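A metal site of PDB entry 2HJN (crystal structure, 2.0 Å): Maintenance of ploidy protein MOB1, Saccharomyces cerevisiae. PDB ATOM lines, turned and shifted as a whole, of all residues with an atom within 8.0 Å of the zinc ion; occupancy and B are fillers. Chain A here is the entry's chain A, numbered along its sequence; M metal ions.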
ATOM      1  N   TYR A  94      14.411  36.553 -20.867  1.00  0.00           N
ATOM      2  CA  TYR A  94      14.639  35.101 -21.187  1.00  0.00           C
ATOM      3  C   TYR A  94      13.681  34.595 -22.225  1.00  0.00           C
ATOM      4  O   TYR A  94      14.045  33.832 -23.136  1.00  0.00           O
ATOM      5  CB  TYR A  94      14.629  34.208 -19.928  1.00  0.00           C
ATOM      6  CG  TYR A  94      15.739  33.182 -19.935  1.00  0.00           C
ATOM      7  CD1 TYR A  94      16.926  33.427 -19.263  1.00  0.00           C
ATOM      8  CD2 TYR A  94      15.610  32.001 -20.645  1.00  0.00           C
ATOM      9  CE1 TYR A  94      17.965  32.501 -19.300  1.00  0.00           C
ATOM     10  CE2 TYR A  94      16.664  31.024 -20.664  1.00  0.00           C
ATOM     11  CZ  TYR A  94      17.828  31.292 -19.996  1.00  0.00           C
ATOM     12  OH  TYR A  94      18.845  30.390 -19.991  1.00  0.00           O
ATOM     13  N   ILE A  97      14.704  35.047 -25.941  1.00  0.00           N
ATOM     14  CA  ILE A  97      15.751  34.185 -26.517  1.00  0.00           C
ATOM     15  C   ILE A  97      15.591  32.693 -26.199  1.00  0.00           C
ATOM     16  O   ILE A  97      16.500  31.899 -26.482  1.00  0.00           O
ATOM     17  CB  ILE A  97      17.179  34.711 -26.179  1.00  0.00           C
ATOM     18  CG1 ILE A  97      17.369  34.990 -24.674  1.00  0.00           C
ATOM     19  CG2 ILE A  97      17.451  35.974 -26.959  1.00  0.00           C
ATOM     20  CD1 ILE A  97      17.802  33.806 -23.844  1.00  0.00           C
ATOM     21  N   THR A  98      14.440  32.335 -25.622  1.00  0.00           N
ATOM     22  CA  THR A  98      14.278  30.988 -25.042  1.00  0.00           C
ATOM     23  C   THR A  98      14.496  29.815 -26.024  1.00  0.00           C
ATOM     24  O   THR A  98      14.980  28.700 -25.619  1.00  0.00           O
ATOM     25  CB  THR A  98      12.867  30.827 -24.392  1.00  0.00           C
ATOM     26  OG1 THR A  98      12.818  29.561 -23.743  1.00  0.00           O
ATOM     27  CG2 THR A  98      11.725  30.867 -25.465  1.00  0.00           C
ATOM     28  N   PHE A 100      16.761  29.618 -28.157  1.00  0.00           N
ATOM     29  CA  PHE A 100      18.226  29.469 -28.361  1.00  0.00           C
ATOM     30  C   PHE A 100      18.952  28.836 -27.160  1.00  0.00           C
ATOM     31  O   PHE A 100      20.152  28.611 -27.198  1.00  0.00           O
ATOM     32  CB  PHE A 100      18.858  30.842 -28.642  1.00  0.00           C
ATOM     33  CG  PHE A 100      18.170  31.604 -29.771  1.00  0.00           C
ATOM     34  CD1 PHE A 100      17.478  32.780 -29.513  1.00  0.00           C
ATOM     35  CD2 PHE A 100      18.181  31.101 -31.066  1.00  0.00           C
ATOM     36  CE1 PHE A 100      16.825  33.474 -30.535  1.00  0.00           C
ATOM     37  CE2 PHE A 100      17.523  31.796 -32.102  1.00  0.00           C
ATOM     38  CZ  PHE A 100      16.846  32.988 -31.832  1.00  0.00           C
ATOM     39  N   CYS A 101      18.194  28.537 -26.101  1.00  0.00           N
ATOM     40  CA  CYS A 101      18.741  27.904 -24.882  1.00  0.00           C
ATOM     41  C   CYS A 101      17.992  26.588 -24.606  1.00  0.00           C
ATOM     42  O   CYS A 101      16.897  26.558 -24.050  1.00  0.00           O
ATOM     43  CB  CYS A 101      18.679  28.862 -23.712  1.00  0.00           C
ATOM     44  SG  CYS A 101      19.396  28.246 -22.188  1.00  0.00           S
ATOM     45  N   SER A 102      18.600  25.491 -25.035  1.00  0.00           N
ATOM     46  CA  SER A 102      18.071  24.130 -24.849  1.00  0.00           C
ATOM     47  C   SER A 102      19.072  23.244 -24.074  1.00  0.00           C
ATOM     48  O   SER A 102      20.202  23.633 -23.854  1.00  0.00           O
ATOM     49  CB  SER A 102      17.786  23.447 -26.208  1.00  0.00           C
ATOM     50  OG  SER A 102      19.005  23.089 -26.845  1.00  0.00           O
ATOM     51  N   PRO A 103      18.632  22.051 -23.617  1.00  0.00           N
ATOM     52  CA  PRO A 103      19.576  21.178 -22.956  1.00  0.00           C
ATOM     53  C   PRO A 103      20.742  20.724 -23.844  1.00  0.00           C
ATOM     54  O   PRO A 103      21.763  20.288 -23.287  1.00  0.00           O
ATOM     55  CB  PRO A 103      18.731  19.981 -22.569  1.00  0.00           C
ATOM     56  CG  PRO A 103      17.416  20.454 -22.480  1.00  0.00           C
ATOM     57  CD  PRO A 103      17.277  21.459 -23.604  1.00  0.00           C
ATOM     58  N   THR A 105      22.187  22.969 -26.350  1.00  0.00           N
ATOM     59  CA  THR A 105      23.137  24.103 -26.451  1.00  0.00           C
ATOM     60  C   THR A 105      23.826  24.375 -25.123  1.00  0.00           C
ATOM     61  O   THR A 105      25.014  24.717 -25.088  1.00  0.00           O
ATOM     62  CB  THR A 105      22.474  25.448 -26.936  1.00  0.00           C
ATOM     63  OG1 THR A 105      21.472  25.857 -25.984  1.00  0.00           O
ATOM     64  CG2 THR A 105      21.834  25.251 -28.316  1.00  0.00           C
ATOM     65  N   CYS A 106      23.084  24.248 -24.032  1.00  0.00           N
ATOM     66  CA  CYS A 106      23.592  24.597 -22.706  1.00  0.00           C
ATOM     67  C   CYS A 106      23.328  23.463 -21.699  1.00  0.00           C
ATOM     68  O   CYS A 106      22.376  23.540 -20.892  1.00  0.00           O
ATOM     69  CB  CYS A 106      22.997  25.969 -22.214  1.00  0.00           C
ATOM     70  SG  CYS A 106      23.093  27.335 -23.418  1.00  0.00           S
ATOM     71  N   PRO A 107      24.219  22.410 -21.708  1.00  0.00           N
ATOM     72  CA  PRO A 107      24.072  21.268 -20.819  1.00  0.00           C
ATOM     73  C   PRO A 107      24.306  21.514 -19.312  1.00  0.00           C
ATOM     74  O   PRO A 107      23.992  20.641 -18.517  1.00  0.00           O
ATOM     75  CB  PRO A 107      25.069  20.220 -21.371  1.00  0.00           C
ATOM     76  CG  PRO A 107      26.004  20.952 -22.230  1.00  0.00           C
ATOM     77  CD  PRO A 107      25.385  22.290 -22.619  1.00  0.00           C
ATOM     78  N   ARG A 108      24.876  22.676 -18.942  1.00  0.00           N
ATOM     79  CA  ARG A 108      25.103  23.042 -17.575  1.00  0.00           C
ATOM     80  C   ARG A 108      24.709  24.525 -17.426  1.00  0.00           C
ATOM     81  O   ARG A 108      24.833  25.330 -18.367  1.00  0.00           O
ATOM     82  CB  ARG A 108      26.577  22.901 -17.184  1.00  0.00           C
ATOM     83  CG  ARG A 108      27.115  21.457 -17.098  1.00  0.00           C
ATOM     84  CD  ARG A 108      28.636  21.514 -16.735  1.00  0.00           C
ATOM     85  NE  ARG A 108      29.405  22.370 -17.655  1.00  0.00           N
ATOM     86  CZ  ARG A 108      30.525  23.046 -17.363  1.00  0.00           C
ATOM     87  NH1 ARG A 108      31.038  22.999 -16.129  1.00  0.00           N
ATOM     88  NH2 ARG A 108      31.130  23.793 -18.300  1.00  0.00           N
ATOM     89  N   MET A 109      24.299  24.897 -16.234  1.00  0.00           N
ATOM     90  CA  MET A 109      23.969  26.319 -15.980  1.00  0.00           C
ATOM     91  C   MET A 109      25.299  27.037 -15.681  1.00  0.00           C
ATOM     92  O   MET A 109      25.767  27.019 -14.548  1.00  0.00           O
ATOM     93  CB  MET A 109      22.937  26.449 -14.843  1.00  0.00           C
ATOM     94  CG  MET A 109      22.589  27.874 -14.454  1.00  0.00           C
ATOM     95  SD  MET A 109      21.668  28.849 -15.910  1.00  0.00           S
ATOM     96  CE  MET A 109      21.180  30.276 -14.686  1.00  0.00           C
ATOM     97  N   ILE A 110      25.887  27.666 -16.696  1.00  0.00           N
ATOM     98  CA  ILE A 110      27.187  28.304 -16.532  1.00  0.00           C
ATOM     99  C   ILE A 110      27.186  29.796 -16.891  1.00  0.00           C
ATOM    100  O   ILE A 110      26.246  30.290 -17.506  1.00  0.00           O
ATOM    101  CB  ILE A 110      28.299  27.536 -17.292  1.00  0.00           C
ATOM    102  CG1 ILE A 110      28.025  27.566 -18.823  1.00  0.00           C
ATOM    103  CG2 ILE A 110      28.322  26.073 -16.777  1.00  0.00           C
ATOM    104  CD1 ILE A 110      29.060  26.944 -19.680  1.00  0.00           C
ATOM    105  N   SER A 131      20.767  21.394 -16.803  1.00  0.00           N
ATOM    106  CA  SER A 131      20.942  22.171 -18.091  1.00  0.00           C
ATOM    107  C   SER A 131      20.497  23.607 -17.787  1.00  0.00           C
ATOM    108  O   SER A 131      19.779  23.799 -16.805  1.00  0.00           O
ATOM    109  CB  SER A 131      20.120  21.539 -19.200  1.00  0.00           C
ATOM    110  OG  SER A 131      18.723  21.777 -19.001  1.00  0.00           O
ATOM    111  N   ALA A 132      20.890  24.609 -18.569  1.00  0.00           N
ATOM    112  CA  ALA A 132      20.521  26.008 -18.237  1.00  0.00           C
ATOM    113  C   ALA A 132      18.993  26.169 -18.258  1.00  0.00           C
ATOM    114  O   ALA A 132      18.429  26.751 -17.362  1.00  0.00           O
ATOM    115  CB  ALA A 132      21.171  27.000 -19.202  1.00  0.00           C
ATOM    116  N   PRO A 133      18.314  25.681 -19.301  1.00  0.00           N
ATOM    117  CA  PRO A 133      16.840  25.929 -19.277  1.00  0.00           C
ATOM    118  C   PRO A 133      16.069  25.193 -18.144  1.00  0.00           C
ATOM    119  O   PRO A 133      15.043  25.695 -17.685  1.00  0.00           O
ATOM    120  CB  PRO A 133      16.399  25.466 -20.650  1.00  0.00           C
ATOM    121  CG  PRO A 133      17.437  24.362 -20.997  1.00  0.00           C
ATOM    122  CD  PRO A 133      18.718  24.944 -20.509  1.00  0.00           C
ATOM    123  N   VAL A 136      16.722  27.491 -15.104  1.00  0.00           N
ATOM    124  CA  VAL A 136      15.968  28.751 -15.198  1.00  0.00           C
ATOM    125  C   VAL A 136      14.479  28.514 -14.924  1.00  0.00           C
ATOM    126  O   VAL A 136      13.872  29.203 -14.081  1.00  0.00           O
ATOM    127  CB  VAL A 136      16.249  29.474 -16.553  1.00  0.00           C
ATOM    128  CG1 VAL A 136      15.385  30.797 -16.684  1.00  0.00           C
ATOM    129  CG2 VAL A 136      17.714  29.820 -16.631  1.00  0.00           C
ATOM    130  N   HIS A 183      23.903  34.152 -16.994  1.00  0.00           N
ATOM    131  CA  HIS A 183      23.824  33.209 -18.135  1.00  0.00           C
ATOM    132  C   HIS A 183      23.512  33.923 -19.479  1.00  0.00           C
ATOM    133  O   HIS A 183      24.069  33.573 -20.531  1.00  0.00           O
ATOM    134  CB  HIS A 183      22.804  32.082 -17.866  1.00  0.00           C
ATOM    135  CG  HIS A 183      22.794  31.030 -18.933  1.00  0.00           C
ATOM    136  ND1 HIS A 183      23.876  30.209 -19.175  1.00  0.00           N
ATOM    137  CD2 HIS A 183      21.906  30.792 -19.929  1.00  0.00           C
ATOM    138  CE1 HIS A 183      23.628  29.474 -20.244  1.00  0.00           C
ATOM    139  NE2 HIS A 183      22.443  29.804 -20.719  1.00  0.00           N
ATOM    140  N   ILE A 184      22.586  34.894 -19.431  1.00  0.00           N
ATOM    141  CA  ILE A 184      22.183  35.635 -20.640  1.00  0.00           C
ATOM    142  C   ILE A 184      23.370  36.353 -21.265  1.00  0.00           C
ATOM    143  O   ILE A 184      23.623  36.237 -22.458  1.00  0.00           O
ATOM    144  CB  ILE A 184      20.979  36.684 -20.400  1.00  0.00           C
ATOM    145  CG1 ILE A 184      19.654  35.987 -20.109  1.00  0.00           C
ATOM    146  CG2 ILE A 184      20.664  37.536 -21.656  1.00  0.00           C
ATOM    147  CD1 ILE A 184      18.634  36.907 -19.437  1.00  0.00           C
ATOM    148  N   CYS A 186      26.706  36.026 -20.717  1.00  0.00           N
ATOM    149  CA  CYS A 186      27.854  35.167 -21.078  1.00  0.00           C
ATOM    150  C   CYS A 186      27.556  34.132 -22.185  1.00  0.00           C
ATOM    151  O   CYS A 186      28.482  33.692 -22.895  1.00  0.00           O
ATOM    152  CB  CYS A 186      28.439  34.470 -19.851  1.00  0.00           C
ATOM    153  SG  CYS A 186      29.040  35.619 -18.587  1.00  0.00           S
ATOM    154  N   HIS A 187      26.306  33.759 -22.368  1.00  0.00           N
ATOM    155  CA  HIS A 187      25.985  32.750 -23.380  1.00  0.00           C
ATOM    156  C   HIS A 187      24.955  33.081 -24.454  1.00  0.00           C
ATOM    157  O   HIS A 187      24.882  32.373 -25.483  1.00  0.00           O
ATOM    158  CB  HIS A 187      25.767  31.391 -22.677  1.00  0.00           C
ATOM    159  CG  HIS A 187      26.972  30.985 -21.879  1.00  0.00           C
ATOM    160  ND1 HIS A 187      28.107  30.492 -22.473  1.00  0.00           N
ATOM    161  CD2 HIS A 187      27.288  31.150 -20.562  1.00  0.00           C
ATOM    162  CE1 HIS A 187      29.035  30.273 -21.553  1.00  0.00           C
ATOM    163  NE2 HIS A 187      28.567  30.694 -20.394  1.00  0.00           N
ATOM    164  N   HIS A 188      24.188  34.169 -24.272  1.00  0.00           N
ATOM    165  CA  HIS A 188      23.167  34.531 -25.284  1.00  0.00           C
ATOM    166  C   HIS A 188      23.189  35.972 -25.787  1.00  0.00           C
ATOM    167  O   HIS A 188      22.227  36.421 -26.400  1.00  0.00           O
ATOM    168  CB  HIS A 188      21.764  34.126 -24.783  1.00  0.00           C
ATOM    169  CG  HIS A 188      21.643  32.657 -24.522  1.00  0.00           C
ATOM    170  ND1 HIS A 188      21.619  31.724 -25.545  1.00  0.00           N
ATOM    171  CD2 HIS A 188      21.717  31.952 -23.372  1.00  0.00           C
ATOM    172  CE1 HIS A 188      21.598  30.506 -25.028  1.00  0.00           C
ATOM    173  NE2 HIS A 188      21.642  30.615 -23.706  1.00  0.00           N
ATOM    174  N   GLU A 191      22.236  36.998 -29.455  1.00  0.00           N
ATOM    175  CA  GLU A 191      20.834  36.813 -29.862  1.00  0.00           C
ATOM    176  C   GLU A 191      20.024  38.012 -29.393  1.00  0.00           C
ATOM    177  O   GLU A 191      19.137  38.456 -30.063  1.00  0.00           O
ATOM    178  CB  GLU A 191      20.316  35.485 -29.305  1.00  0.00           C
ATOM    179  CG  GLU A 191      20.860  34.227 -30.074  1.00  0.00           C
ATOM    180  CD  GLU A 191      21.469  33.160 -29.169  1.00  0.00           C
ATOM    181  OE1 GLU A 191      21.457  33.315 -27.935  1.00  0.00           O
ATOM    182  OE2 GLU A 191      21.974  32.144 -29.680  1.00  0.00           O
HETATM  183 ZN    ZN M   1      21.652  28.929 -22.507  1.00  0.00          ZN
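The side-chain sulfur (SG) of Cys 101 sits close to the side-chain hydroxyl (OH) of Tyr 94 (3.1 Å). The backbone NH (N) of Ala 132 lies within hydrogen-bond range of the backbone carbonyl oxygen (O) of Cys 106. A ring nitrogen (ND1) of His 183 sits at hydrogen-bond distance from the backbone carbonyl oxygen of Ile 110 (2.9 Å). The side-chain hydroxyl (OG1) of Thr 105 sits close to the side-chain sulfur (SG) of Cys 106, at 3.4 Å. A ring nitrogen (ND1) of His 188 lies within hydrogen-bond range of the side-chain carboxylate (OE1) of Glu 191, 2.9 Å away.
Ala 132 touches the zinc ion. Of the 23 residues printed, 5 come within 4 Å of the zinc ion. Along chain A the residues within 4 Å of the zinc ion span positions 101 to 188.
NE2 of His 188 binds the zinc ion, at 2.1 Å. NE2 of His 183 is bound to the zinc ion. The zinc ion is bound by the side-chain sulfur (SG) of Cys 106 (2.3 Å). The zinc ion is bound by SG of Cys 101 (2.4 Å).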
